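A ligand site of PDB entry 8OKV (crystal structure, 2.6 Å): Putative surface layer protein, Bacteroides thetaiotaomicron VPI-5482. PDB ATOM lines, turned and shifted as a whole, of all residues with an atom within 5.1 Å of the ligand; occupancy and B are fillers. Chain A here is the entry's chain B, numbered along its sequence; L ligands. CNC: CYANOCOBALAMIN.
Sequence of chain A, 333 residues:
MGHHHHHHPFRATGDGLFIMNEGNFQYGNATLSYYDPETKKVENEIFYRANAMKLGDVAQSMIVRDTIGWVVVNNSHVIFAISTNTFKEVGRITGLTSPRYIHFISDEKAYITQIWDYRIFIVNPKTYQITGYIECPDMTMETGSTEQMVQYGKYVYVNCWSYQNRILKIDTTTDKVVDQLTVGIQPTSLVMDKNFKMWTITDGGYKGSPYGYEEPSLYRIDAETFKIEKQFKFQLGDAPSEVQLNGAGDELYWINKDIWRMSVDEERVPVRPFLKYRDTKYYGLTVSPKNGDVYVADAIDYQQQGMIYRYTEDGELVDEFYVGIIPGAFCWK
O of Gly 23 is in hydrogen-bond range of N62 of the ligand (2.7 Å).
The side-chain amide oxygen (OD1) of Asn 74 is in hydrogen-bond range of a nitrogen (N33) of the ligand, 2.9 Å away.
O28 of the ligand lies within hydrogen-bond range of NH2 of Arg 100, at 2.9 Å.
NE1 of Trp 116 is in hydrogen-bond range of O34 of the ligand.
NE2 of Gln 186 sits at hydrogen-bond distance from O39 of the ligand, 3.0 Å away.
A nitrogen (N29) of the ligand sits at hydrogen-bond distance from the side-chain carboxylate (OE1) of Glu 22 (3.1 Å).
An oxygen (O63) of the ligand sits at hydrogen-bond distance from the backbone NH of Phe 25.
The side-chain amide oxygen of Gln 60 sits at hydrogen-bond distance from a nitrogen (N29) of the ligand, 3.2 Å away.
The side-chain hydroxyl (OG) of Ser 162 is in hydrogen-bond range of a nitrogen (N40) of the ligand (3.3 Å).
A nitrogen (N33) of the ligand is in hydrogen-bond range of the side-chain hydroxyl (OG) of Ser 98 (3.4 Å).
The side-chain amide nitrogen (ND2) of Asn 74 lies close to the guanidinium group (NH2) of Arg 100, 3.3 Å away.
The side-chain hydroxyl of Ser 98 sits at hydrogen-bond distance from the side-chain amide nitrogen of Asn 74 (2.9 Å).
N of Asn 74 is in hydrogen-bond range of O of Val 58 (2.8 Å).
OE1 of Gln 186 is in hydrogen-bond range of N of Tyr 163.
The side-chain hydroxyl of Tyr 283 is in hydrogen-bond range of the side-chain carboxylate of Glu 22.
O of Ile 326 is in hydrogen-bond range of N of Glu 22 (2.8 Å).
The side-chain hydroxyl (OH) of Tyr 163 sits at hydrogen-bond distance from the side-chain hydroxyl (OH) of Tyr 206.
O of Tyr 302 is in hydrogen-bond range of ND2 of Asn 24 (3.1 Å).
Residues that only touch the ligand: Asn 24 (3.3 Å), Tyr 27 (3.7 Å), Val 58 (3.4 Å), Ile 115 (3.5 Å), Trp 161 (3.4 Å), Tyr 163 (3.6 Å), Tyr 206 (3.3 Å), Tyr 283 (3.5 Å), Tyr 302 (3.6 Å) and Ile 326 (3.6 Å).
Within 4 Å of the ligand: Glu 22, Gly 23, Asn 24, Phe 25, Tyr 27, Val 58, Gln 60, Asn 74, Ser 98, Arg 100, Ile 115, Trp 116, Trp 161, Ser 162, Tyr 163, Gln 186, Tyr 206, Tyr 283, Tyr 302 and Ile 326.
Along chain A the residues within 4 Å of the ligand span positions 22 to 326.
The nearest printed residue that does not touch the ligand is Gln 303 (4.03 Å).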
ATOM      1  N   GLU A  22     -15.712  16.890  27.378  1.00  0.00           N
ATOM      2  CA  GLU A  22     -16.850  16.736  26.478  1.00  0.00           C
ATOM      3  C   GLU A  22     -17.251  18.089  25.863  1.00  0.00           C
ATOM      4  O   GLU A  22     -17.642  18.221  24.698  1.00  0.00           O
ATOM      5  CB  GLU A  22     -18.007  16.041  27.217  1.00  0.00           C
ATOM      6  CG  GLU A  22     -17.668  14.565  27.618  1.00  0.00           C
ATOM      7  CD  GLU A  22     -18.822  13.748  28.163  1.00  0.00           C
ATOM      8  OE1 GLU A  22     -19.927  14.404  28.396  1.00  0.00           O
ATOM      9  OE2 GLU A  22     -18.653  12.476  28.434  1.00  0.00           O
ATOM     10  N   GLY A  23     -17.148  19.110  26.679  1.00  0.00           N
ATOM     11  CA  GLY A  23     -17.741  20.370  26.315  1.00  0.00           C
ATOM     12  C   GLY A  23     -19.263  20.278  26.435  1.00  0.00           C
ATOM     13  O   GLY A  23     -19.840  19.259  26.845  1.00  0.00           O
ATOM     14  N   ASN A  24     -19.869  21.405  26.080  1.00  0.00           N
ATOM     15  CA  ASN A  24     -21.302  21.526  26.011  1.00  0.00           C
ATOM     16  C   ASN A  24     -21.692  20.840  24.703  1.00  0.00           C
ATOM     17  O   ASN A  24     -21.031  20.981  23.669  1.00  0.00           O
ATOM     18  CB  ASN A  24     -21.692  22.987  26.303  1.00  0.00           C
ATOM     19  CG  ASN A  24     -21.433  23.355  27.754  1.00  0.00           C
ATOM     20  OD1 ASN A  24     -20.605  24.212  28.052  1.00  0.00           O
ATOM     21  ND2 ASN A  24     -22.151  22.687  28.655  1.00  0.00           N
ATOM     22  N   PHE A  25     -22.648  19.919  24.850  1.00  0.00           N
ATOM     23  CA  PHE A  25     -23.261  19.208  23.732  1.00  0.00           C
ATOM     24  C   PHE A  25     -23.967  20.240  22.865  1.00  0.00           C
ATOM     25  O   PHE A  25     -24.710  21.050  23.413  1.00  0.00           O
ATOM     26  CB  PHE A  25     -24.266  18.206  24.289  1.00  0.00           C
ATOM     27  CG  PHE A  25     -25.221  17.617  23.284  1.00  0.00           C
ATOM     28  CD1 PHE A  25     -24.752  16.864  22.219  1.00  0.00           C
ATOM     29  CD2 PHE A  25     -26.599  17.791  23.441  1.00  0.00           C
ATOM     30  CE1 PHE A  25     -25.646  16.290  21.324  1.00  0.00           C
ATOM     31  CE2 PHE A  25     -27.484  17.256  22.525  1.00  0.00           C
ATOM     32  CZ  PHE A  25     -27.000  16.507  21.473  1.00  0.00           C
ATOM     33  N   TYR A  27     -22.569  22.772  21.410  1.00  0.00           N
ATOM     34  CA  TYR A  27     -21.874  24.077  21.422  1.00  0.00           C
ATOM     35  C   TYR A  27     -20.475  24.020  20.786  1.00  0.00           C
ATOM     36  O   TYR A  27     -19.846  25.080  20.654  1.00  0.00           O
ATOM     37  CB  TYR A  27     -21.819  24.680  22.833  1.00  0.00           C
ATOM     38  CG  TYR A  27     -23.096  25.286  23.374  1.00  0.00           C
ATOM     39  CD1 TYR A  27     -24.203  24.470  23.580  1.00  0.00           C
ATOM     40  CD2 TYR A  27     -23.229  26.657  23.623  1.00  0.00           C
ATOM     41  CE1 TYR A  27     -25.409  24.976  24.028  1.00  0.00           C
ATOM     42  CE2 TYR A  27     -24.429  27.180  24.104  1.00  0.00           C
ATOM     43  CZ  TYR A  27     -25.526  26.330  24.280  1.00  0.00           C
ATOM     44  OH  TYR A  27     -26.742  26.737  24.751  1.00  0.00           O
ATOM     45  N   VAL A  58     -18.812  16.415  21.005  1.00  0.00           N
ATOM     46  CA  VAL A  58     -18.755  15.750  22.326  1.00  0.00           C
ATOM     47  C   VAL A  58     -17.551  14.812  22.366  1.00  0.00           C
ATOM     48  O   VAL A  58     -17.697  13.687  21.884  1.00  0.00           O
ATOM     49  CB  VAL A  58     -20.087  15.059  22.712  1.00  0.00           C
ATOM     50  CG1 VAL A  58     -19.962  14.053  23.830  1.00  0.00           C
ATOM     51  CG2 VAL A  58     -21.145  16.081  23.091  1.00  0.00           C
ATOM     52  N   GLN A  60     -15.456  12.115  23.554  1.00  0.00           N
ATOM     53  CA  GLN A  60     -16.002  11.070  24.405  1.00  0.00           C
ATOM     54  C   GLN A  60     -14.904  10.209  25.052  1.00  0.00           C
ATOM     55  O   GLN A  60     -15.032   9.878  26.238  1.00  0.00           O
ATOM     56  CB  GLN A  60     -16.912  10.190  23.526  1.00  0.00           C
ATOM     57  CG  GLN A  60     -17.613   9.079  24.263  1.00  0.00           C
ATOM     58  CD  GLN A  60     -18.389   9.564  25.469  1.00  0.00           C
ATOM     59  OE1 GLN A  60     -19.077  10.586  25.399  1.00  0.00           O
ATOM     60  NE2 GLN A  60     -18.273   8.841  26.575  1.00  0.00           N
ATOM     61  N   ASN A  74     -17.722  12.166  19.513  1.00  0.00           N
ATOM     62  CA  ASN A  74     -19.075  11.635  19.393  1.00  0.00           C
ATOM     63  C   ASN A  74     -19.976  12.465  18.479  1.00  0.00           C
ATOM     64  O   ASN A  74     -20.663  11.910  17.625  1.00  0.00           O
ATOM     65  CB  ASN A  74     -19.744  11.469  20.775  1.00  0.00           C
ATOM     66  CG  ASN A  74     -21.251  11.233  20.754  1.00  0.00           C
ATOM     67  OD1 ASN A  74     -22.047  12.138  20.986  1.00  0.00           O
ATOM     68  ND2 ASN A  74     -21.685   9.996  20.543  1.00  0.00           N
ATOM     69  N   ASN A  75     -20.073  13.768  18.724  1.00  0.00           N
ATOM     70  CA  ASN A  75     -21.042  14.593  18.021  1.00  0.00           C
ATOM     71  C   ASN A  75     -20.356  15.426  16.958  1.00  0.00           C
ATOM     72  O   ASN A  75     -20.916  16.445  16.597  1.00  0.00           O
ATOM     73  CB  ASN A  75     -21.849  15.520  18.953  1.00  0.00           C
ATOM     74  CG  ASN A  75     -23.085  16.144  18.328  1.00  0.00           C
ATOM     75  OD1 ASN A  75     -23.756  15.516  17.507  1.00  0.00           O
ATOM     76  ND2 ASN A  75     -23.458  17.385  18.635  1.00  0.00           N
ATOM     77  N   SER A  98     -22.568   8.432  15.380  1.00  0.00           N
ATOM     78  CA  SER A  98     -22.401   9.172  16.615  1.00  0.00           C
ATOM     79  C   SER A  98     -21.552   8.312  17.564  1.00  0.00           C
ATOM     80  O   SER A  98     -22.055   7.733  18.551  1.00  0.00           O
ATOM     81  CB  SER A  98     -23.726   9.574  17.191  1.00  0.00           C
ATOM     82  OG  SER A  98     -23.557  10.393  18.340  1.00  0.00           O
ATOM     83  N   ARG A 100     -18.695   6.326  20.022  1.00  0.00           N
ATOM     84  CA  ARG A 100     -18.613   6.213  21.459  1.00  0.00           C
ATOM     85  C   ARG A 100     -17.195   5.778  21.860  1.00  0.00           C
ATOM     86  O   ARG A 100     -16.482   6.535  22.508  1.00  0.00           O
ATOM     87  CB  ARG A 100     -19.746   5.262  21.853  1.00  0.00           C
ATOM     88  CG  ARG A 100     -21.150   5.672  21.412  1.00  0.00           C
ATOM     89  CD  ARG A 100     -21.685   6.959  21.989  1.00  0.00           C
ATOM     90  NE  ARG A 100     -21.824   6.927  23.447  1.00  0.00           N
ATOM     91  CZ  ARG A 100     -21.870   8.002  24.259  1.00  0.00           C
ATOM     92  NH1 ARG A 100     -21.851   7.821  25.573  1.00  0.00           N
ATOM     93  NH2 ARG A 100     -21.939   9.228  23.756  1.00  0.00           N
ATOM     94  N   ILE A 115     -24.095   5.625  19.302  1.00  0.00           N
ATOM     95  CA  ILE A 115     -25.451   5.930  19.745  1.00  0.00           C
ATOM     96  C   ILE A 115     -26.250   6.380  18.497  1.00  0.00           C
ATOM     97  O   ILE A 115     -25.641   6.751  17.470  1.00  0.00           O
ATOM     98  CB  ILE A 115     -25.439   6.902  20.946  1.00  0.00           C
ATOM     99  CG1 ILE A 115     -26.827   7.002  21.589  1.00  0.00           C
ATOM    100  CG2 ILE A 115     -24.899   8.276  20.549  1.00  0.00           C
ATOM    101  CD1 ILE A 115     -26.935   7.858  22.848  1.00  0.00           C
ATOM    102  N   TRP A 116     -27.607   6.245  18.555  1.00  0.00           N
ATOM    103  CA  TRP A 116     -28.515   6.585  17.458  1.00  0.00           C
ATOM    104  C   TRP A 116     -28.274   5.742  16.185  1.00  0.00           C
ATOM    105  O   TRP A 116     -28.398   6.257  15.056  1.00  0.00           O
ATOM    106  CB  TRP A 116     -28.519   8.077  17.109  1.00  0.00           C
ATOM    107  CG  TRP A 116     -28.633   8.963  18.306  1.00  0.00           C
ATOM    108  CD1 TRP A 116     -27.771   9.978  18.612  1.00  0.00           C
ATOM    109  CD2 TRP A 116     -29.576   8.891  19.401  1.00  0.00           C
ATOM    110  NE1 TRP A 116     -28.122  10.541  19.812  1.00  0.00           N
ATOM    111  CE2 TRP A 116     -29.218   9.898  20.319  1.00  0.00           C
ATOM    112  CE3 TRP A 116     -30.670   8.071  19.701  1.00  0.00           C
ATOM    113  CZ2 TRP A 116     -29.931  10.122  21.502  1.00  0.00           C
ATOM    114  CZ3 TRP A 116     -31.362   8.289  20.891  1.00  0.00           C
ATOM    115  CH2 TRP A 116     -31.031   9.324  21.755  1.00  0.00           C
ATOM    116  N   TRP A 161     -26.381   1.134  26.182  1.00  0.00           N
ATOM    117  CA  TRP A 161     -26.715   2.128  27.196  1.00  0.00           C
ATOM    118  C   TRP A 161     -28.061   2.894  26.952  1.00  0.00           C
ATOM    119  O   TRP A 161     -29.066   2.525  27.582  1.00  0.00           O
ATOM    120  CB  TRP A 161     -25.508   3.033  27.337  1.00  0.00           C
ATOM    121  CG  TRP A 161     -25.792   4.219  28.181  1.00  0.00           C
ATOM    122  CD1 TRP A 161     -26.225   4.200  29.489  1.00  0.00           C
ATOM    123  CD2 TRP A 161     -25.664   5.605  27.839  1.00  0.00           C
ATOM    124  NE1 TRP A 161     -26.415   5.467  29.950  1.00  0.00           N
ATOM    125  CE2 TRP A 161     -26.044   6.361  28.987  1.00  0.00           C
ATOM    126  CE3 TRP A 161     -25.266   6.300  26.692  1.00  0.00           C
ATOM    127  CZ2 TRP A 161     -26.077   7.756  28.999  1.00  0.00           C
ATOM    128  CZ3 TRP A 161     -25.262   7.680  26.713  1.00  0.00           C
ATOM    129  CH2 TRP A 161     -25.681   8.400  27.854  1.00  0.00           C
ATOM    130  N   SER A 162     -28.074   3.981  26.126  1.00  0.00           N
ATOM    131  CA  SER A 162     -29.238   4.865  25.921  1.00  0.00           C
ATOM    132  C   SER A 162     -30.437   4.054  25.412  1.00  0.00           C
ATOM    133  O   SER A 162     -30.403   3.548  24.283  1.00  0.00           O
ATOM    134  CB  SER A 162     -28.942   6.071  24.979  1.00  0.00           C
ATOM    135  OG  SER A 162     -30.101   6.639  24.333  1.00  0.00           O
ATOM    136  N   TYR A 163     -31.436   3.883  26.311  1.00  0.00           N
ATOM    137  CA  TYR A 163     -32.698   3.219  25.994  1.00  0.00           C
ATOM    138  C   TYR A 163     -32.457   1.761  25.577  1.00  0.00           C
ATOM    139  O   TYR A 163     -33.125   1.259  24.656  1.00  0.00           O
ATOM    140  CB  TYR A 163     -33.468   4.016  24.917  1.00  0.00           C
ATOM    141  CG  TYR A 163     -33.671   5.501  25.164  1.00  0.00           C
ATOM    142  CD1 TYR A 163     -34.138   5.973  26.383  1.00  0.00           C
ATOM    143  CD2 TYR A 163     -33.455   6.431  24.148  1.00  0.00           C
ATOM    144  CE1 TYR A 163     -34.372   7.337  26.593  1.00  0.00           C
ATOM    145  CE2 TYR A 163     -33.668   7.795  24.351  1.00  0.00           C
ATOM    146  CZ  TYR A 163     -34.134   8.248  25.574  1.00  0.00           C
ATOM    147  OH  TYR A 163     -34.325   9.589  25.743  1.00  0.00           O
ATOM    148  N   GLN A 186     -30.026   0.643  30.967  1.00  0.00           N
ATOM    149  CA  GLN A 186     -28.967   1.588  30.640  1.00  0.00           C
ATOM    150  C   GLN A 186     -27.714   1.205  31.418  1.00  0.00           C
ATOM    151  O   GLN A 186     -27.271   1.931  32.309  1.00  0.00           O
ATOM    152  CB  GLN A 186     -29.494   3.032  30.861  1.00  0.00           C
ATOM    153  CG  GLN A 186     -30.859   3.319  30.202  1.00  0.00           C
ATOM    154  CD  GLN A 186     -31.276   4.766  30.046  1.00  0.00           C
ATOM    155  OE1 GLN A 186     -32.285   5.114  29.388  1.00  0.00           O
ATOM    156  NE2 GLN A 186     -30.579   5.636  30.769  1.00  0.00           N
ATOM    157  N   TYR A 206     -33.823   8.170  34.126  1.00  0.00           N
ATOM    158  CA  TYR A 206     -34.051   9.499  34.686  1.00  0.00           C
ATOM    159  C   TYR A 206     -35.546   9.689  34.952  1.00  0.00           C
ATOM    160  O   TYR A 206     -36.390   9.044  34.339  1.00  0.00           O
ATOM    161  CB  TYR A 206     -33.500  10.593  33.755  1.00  0.00           C
ATOM    162  CG  TYR A 206     -33.998  10.610  32.333  1.00  0.00           C
ATOM    163  CD1 TYR A 206     -33.528   9.704  31.387  1.00  0.00           C
ATOM    164  CD2 TYR A 206     -34.957  11.533  31.908  1.00  0.00           C
ATOM    165  CE1 TYR A 206     -33.986   9.722  30.071  1.00  0.00           C
ATOM    166  CE2 TYR A 206     -35.409  11.573  30.596  1.00  0.00           C
ATOM    167  CZ  TYR A 206     -34.924  10.661  29.664  1.00  0.00           C
ATOM    168  OH  TYR A 206     -35.438  10.686  28.363  1.00  0.00           O
ATOM    169  N   TYR A 283     -17.889  12.945  37.405  1.00  0.00           N
ATOM    170  CA  TYR A 283     -18.431  12.615  36.071  1.00  0.00           C
ATOM    171  C   TYR A 283     -17.521  11.663  35.290  1.00  0.00           C
ATOM    172  O   TYR A 283     -18.052  10.831  34.556  1.00  0.00           O
ATOM    173  CB  TYR A 283     -18.726  13.889  35.272  1.00  0.00           C
ATOM    174  CG  TYR A 283     -19.446  13.694  33.957  1.00  0.00           C
ATOM    175  CD1 TYR A 283     -20.775  13.308  33.891  1.00  0.00           C
ATOM    176  CD2 TYR A 283     -18.801  13.908  32.754  1.00  0.00           C
ATOM    177  CE1 TYR A 283     -21.441  13.199  32.689  1.00  0.00           C
ATOM    178  CE2 TYR A 283     -19.435  13.758  31.529  1.00  0.00           C
ATOM    179  CZ  TYR A 283     -20.775  13.414  31.478  1.00  0.00           C
ATOM    180  OH  TYR A 283     -21.492  13.247  30.273  1.00  0.00           O
ATOM    181  N   ASP A 301     -21.449  21.546  38.111  1.00  0.00           N
ATOM    182  CA  ASP A 301     -22.493  22.359  37.449  1.00  0.00           C
ATOM    183  C   ASP A 301     -22.553  22.224  35.909  1.00  0.00           C
ATOM    184  O   ASP A 301     -23.526  22.761  35.384  1.00  0.00           O
ATOM    185  CB  ASP A 301     -22.528  23.849  37.918  1.00  0.00           C
ATOM    186  CG  ASP A 301     -21.705  24.976  37.253  1.00  0.00           C
ATOM    187  OD1 ASP A 301     -20.904  24.765  36.274  1.00  0.00           O
ATOM    188  OD2 ASP A 301     -21.856  26.087  37.733  1.00  0.00           O
ATOM    189  N   TYR A 302     -21.673  21.456  35.214  1.00  0.00           N
ATOM    190  CA  TYR A 302     -21.706  21.235  33.760  1.00  0.00           C
ATOM    191  C   TYR A 302     -21.620  22.510  32.892  1.00  0.00           C
ATOM    192  O   TYR A 302     -21.868  22.420  31.696  1.00  0.00           O
ATOM    193  CB  TYR A 302     -22.974  20.513  33.346  1.00  0.00           C
ATOM    194  CG  TYR A 302     -23.301  19.226  34.058  1.00  0.00           C
ATOM    195  CD1 TYR A 302     -22.480  18.124  33.915  1.00  0.00           C
ATOM    196  CD2 TYR A 302     -24.510  19.058  34.748  1.00  0.00           C
ATOM    197  CE1 TYR A 302     -22.828  16.888  34.455  1.00  0.00           C
ATOM    198  CE2 TYR A 302     -24.859  17.849  35.326  1.00  0.00           C
ATOM    199  CZ  TYR A 302     -24.032  16.741  35.148  1.00  0.00           C
ATOM    200  OH  TYR A 302     -24.419  15.561  35.744  1.00  0.00           O
ATOM    201  N   GLN A 303     -21.254  23.671  33.440  1.00  0.00           N
ATOM    202  CA  GLN A 303     -21.288  24.947  32.720  1.00  0.00           C
ATOM    203  C   GLN A 303     -19.909  25.561  32.711  1.00  0.00           C
ATOM    204  O   GLN A 303     -19.383  25.886  31.651  1.00  0.00           O
ATOM    205  CB  GLN A 303     -22.221  25.986  33.364  1.00  0.00           C
ATOM    206  CG  GLN A 303     -23.715  25.796  33.120  1.00  0.00           C
ATOM    207  CD  GLN A 303     -24.559  25.936  34.377  1.00  0.00           C
ATOM    208  OE1 GLN A 303     -24.363  26.830  35.219  1.00  0.00           O
ATOM    209  NE2 GLN A 303     -25.466  24.977  34.572  1.00  0.00           N
ATOM    210  N   ILE A 326     -16.811  20.107  31.243  1.00  0.00           N
ATOM    211  CA  ILE A 326     -17.291  18.734  31.408  1.00  0.00           C
ATOM    212  C   ILE A 326     -16.198  17.716  31.035  1.00  0.00           C
ATOM    213  O   ILE A 326     -16.354  16.947  30.113  1.00  0.00           O
ATOM    214  CB  ILE A 326     -18.618  18.480  30.653  1.00  0.00           C
ATOM    215  CG1 ILE A 326     -19.713  19.529  30.913  1.00  0.00           C
ATOM    216  CG2 ILE A 326     -19.159  17.073  30.968  1.00  0.00           C
ATOM    217  CD1 ILE A 326     -20.863  19.496  29.886  1.00  0.00           C
HETATM  218 CO   CNC L   1     -27.785  13.646  28.673  1.00  0.00          CO
HETATM  219  N21 CNC L   1     -26.631  13.411  27.299  1.00  0.00           N
HETATM  220  N22 CNC L   1     -28.958  12.366  27.954  1.00  0.00           N
HETATM  221  N23 CNC L   1     -28.789  13.898  30.225  1.00  0.00           N
HETATM  222  N24 CNC L   1     -26.434  14.772  29.318  1.00  0.00           N
HETATM  223  C1  CNC L   1     -25.598  14.424  27.163  1.00  0.00           C
HETATM  224  C20 CNC L   1     -26.178  15.716  26.549  1.00  0.00           C
HETATM  225  C2  CNC L   1     -24.484  13.570  26.403  1.00  0.00           C
HETATM  226  C25 CNC L   1     -23.571  14.459  25.588  1.00  0.00           C
HETATM  227  C26 CNC L   1     -23.643  12.633  27.322  1.00  0.00           C
HETATM  228  C27 CNC L   1     -22.555  11.844  26.602  1.00  0.00           C
HETATM  229  O28 CNC L   1     -22.686  10.667  26.164  1.00  0.00           O
HETATM  230  N29 CNC L   1     -21.428  12.515  26.491  1.00  0.00           N
HETATM  231  C3  CNC L   1     -25.327  12.604  25.564  1.00  0.00           C
HETATM  232  C30 CNC L   1     -25.822  13.089  24.201  1.00  0.00           C
HETATM  233  C31 CNC L   1     -24.892  12.836  23.002  1.00  0.00           C
HETATM  234  C32 CNC L   1     -25.644  12.505  21.746  1.00  0.00           C
HETATM  235  O34 CNC L   1     -26.845  12.306  21.802  1.00  0.00           O
HETATM  236  N33 CNC L   1     -24.914  12.428  20.639  1.00  0.00           N
HETATM  237  C4  CNC L   1     -26.556  12.443  26.440  1.00  0.00           C
HETATM  238  C5  CNC L   1     -27.541  11.346  26.337  1.00  0.00           C
HETATM  239  C35 CNC L   1     -27.181  10.204  25.398  1.00  0.00           C
HETATM  240  C6  CNC L   1     -28.707  11.391  27.055  1.00  0.00           C
HETATM  241  C7  CNC L   1     -29.882  10.433  27.000  1.00  0.00           C
HETATM  242  C36 CNC L   1     -30.219   9.880  25.596  1.00  0.00           C
HETATM  243  C37 CNC L   1     -29.518   9.316  27.963  1.00  0.00           C
HETATM  244  C38 CNC L   1     -30.566   8.267  28.264  1.00  0.00           C
HETATM  245  O39 CNC L   1     -31.063   8.275  29.347  1.00  0.00           O
HETATM  246  N40 CNC L   1     -30.921   7.279  27.457  1.00  0.00           N
HETATM  247  C8  CNC L   1     -31.013  11.321  27.482  1.00  0.00           C
HETATM  248  C41 CNC L   1     -31.877  12.162  26.493  1.00  0.00           C
HETATM  249  C42 CNC L   1     -33.200  12.730  27.021  1.00  0.00           C
HETATM  250  C43 CNC L   1     -33.646  14.033  26.380  1.00  0.00           C
HETATM  251  O44 CNC L   1     -34.312  14.825  27.014  1.00  0.00           O
HETATM  252  N45 CNC L   1     -33.330  14.303  25.127  1.00  0.00           N
HETATM  253  C9  CNC L   1     -30.162  12.207  28.319  1.00  0.00           C
HETATM  254  C10 CNC L   1     -30.729  12.683  29.570  1.00  0.00           C
HETATM  255  C11 CNC L   1     -29.988  13.304  30.483  1.00  0.00           C
HETATM  256  C12 CNC L   1     -30.373  13.304  31.944  1.00  0.00           C
HETATM  257  C46 CNC L   1     -31.899  13.316  32.204  1.00  0.00           C
HETATM  258  C47 CNC L   1     -29.780  12.024  32.555  1.00  0.00           C
HETATM  259  C13 CNC L   1     -29.599  14.563  32.305  1.00  0.00           C
HETATM  260  C48 CNC L   1     -30.449  15.846  32.261  1.00  0.00           C
HETATM  261  C49 CNC L   1     -31.191  16.185  33.547  1.00  0.00           C
HETATM  262  C50 CNC L   1     -31.000  17.674  33.544  1.00  0.00           C
HETATM  263  O51 CNC L   1     -30.120  18.095  34.257  1.00  0.00           O
HETATM  264  N52 CNC L   1     -31.739  18.407  32.678  1.00  0.00           N
HETATM  265  C14 CNC L   1     -28.494  14.667  31.235  1.00  0.00           C
HETATM  266  C15 CNC L   1     -27.296  15.565  31.343  1.00  0.00           C
HETATM  267  C53 CNC L   1     -27.250  16.545  32.505  1.00  0.00           C
HETATM  268  C16 CNC L   1     -26.314  15.502  30.455  1.00  0.00           C
HETATM  269  C17 CNC L   1     -24.928  16.164  30.546  1.00  0.00           C
HETATM  270  C54 CNC L   1     -24.156  15.311  31.532  1.00  0.00           C
HETATM  271  C55 CNC L   1     -24.805  17.695  30.846  1.00  0.00           C
HETATM  272  C56 CNC L   1     -25.874  18.571  30.088  1.00  0.00           C
HETATM  273  C57 CNC L   1     -26.223  19.796  30.841  1.00  0.00           C
HETATM  274  O58 CNC L   1     -27.011  19.591  31.760  1.00  0.00           O
HETATM  275  N59 CNC L   1     -25.553  20.907  30.499  1.00  0.00           N
HETATM  276  C18 CNC L   1     -24.520  16.013  29.088  1.00  0.00           C
HETATM  277  C60 CNC L   1     -23.005  16.010  28.762  1.00  0.00           C
HETATM  278  C61 CNC L   1     -22.579  17.124  27.795  1.00  0.00           C
HETATM  279  O63 CNC L   1     -23.261  18.086  27.419  1.00  0.00           O
HETATM  280  N62 CNC L   1     -21.300  17.016  27.365  1.00  0.00           N
HETATM  281  C19 CNC L   1     -25.459  14.963  28.560  1.00  0.00           C
HETATM  282  C1P CNC L   1     -25.541  22.073  31.387  1.00  0.00           C
HETATM  283  C2P CNC L   1     -26.082  23.290  30.663  1.00  0.00           C
HETATM  284  C3P CNC L   1     -25.016  23.914  29.802  1.00  0.00           C
HETATM  285  O3  CNC L   1     -27.174  22.926  29.818  1.00  0.00           O
HETATM  286  O4  CNC L   1     -28.990  23.326  28.036  1.00  0.00           O
HETATM  287  O5  CNC L   1     -26.720  23.625  27.220  1.00  0.00           O
HETATM  288  P   CNC L   1     -27.564  22.845  28.215  1.00  0.00           P
HETATM  289  O2  CNC L   1     -27.856  21.281  28.019  1.00  0.00           O
HETATM  290  C3R CNC L   1     -29.208  20.742  28.036  1.00  0.00           C
HETATM  291  C2R CNC L   1     -29.174  19.468  27.265  1.00  0.00           C
HETATM  292  O7R CNC L   1     -27.859  18.830  27.309  1.00  0.00           O
HETATM  293  C1R CNC L   1     -30.328  18.686  27.904  1.00  0.00           C
HETATM  294  O6R CNC L   1     -30.401  19.065  29.278  1.00  0.00           O
HETATM  295  C4R CNC L   1     -29.814  20.377  29.407  1.00  0.00           C
HETATM  296  C5R CNC L   1     -30.910  21.328  29.877  1.00  0.00           C
HETATM  297  O8R CNC L   1     -30.349  22.625  30.189  1.00  0.00           O
HETATM  298  N1B CNC L   1     -29.970  17.278  27.647  1.00  0.00           N
HETATM  299  C8B CNC L   1     -30.103  16.715  26.476  1.00  0.00           C
HETATM  300  C2B CNC L   1     -29.358  16.454  28.483  1.00  0.00           C
HETATM  301  N3B CNC L   1     -29.098  15.278  27.903  1.00  0.00           N
HETATM  302  C9B CNC L   1     -29.575  15.380  26.675  1.00  0.00           C
HETATM  303  C4B CNC L   1     -29.637  14.537  25.612  1.00  0.00           C
HETATM  304  C5B CNC L   1     -30.142  14.926  24.409  1.00  0.00           C
HETATM  305  C5M CNC L   1     -30.061  13.834  23.412  1.00  0.00           C
HETATM  306  C6B CNC L   1     -30.695  16.270  24.159  1.00  0.00           C
HETATM  307  C6M CNC L   1     -31.256  16.711  22.819  1.00  0.00           C
HETATM  308  C7B CNC L   1     -30.642  17.135  25.239  1.00  0.00           C
HETATM  309  N1A CNC L   1     -27.414  11.199  30.224  1.00  0.00           N
HETATM  310  C1A CNC L   1     -27.399  12.167  29.581  1.00  0.00           C
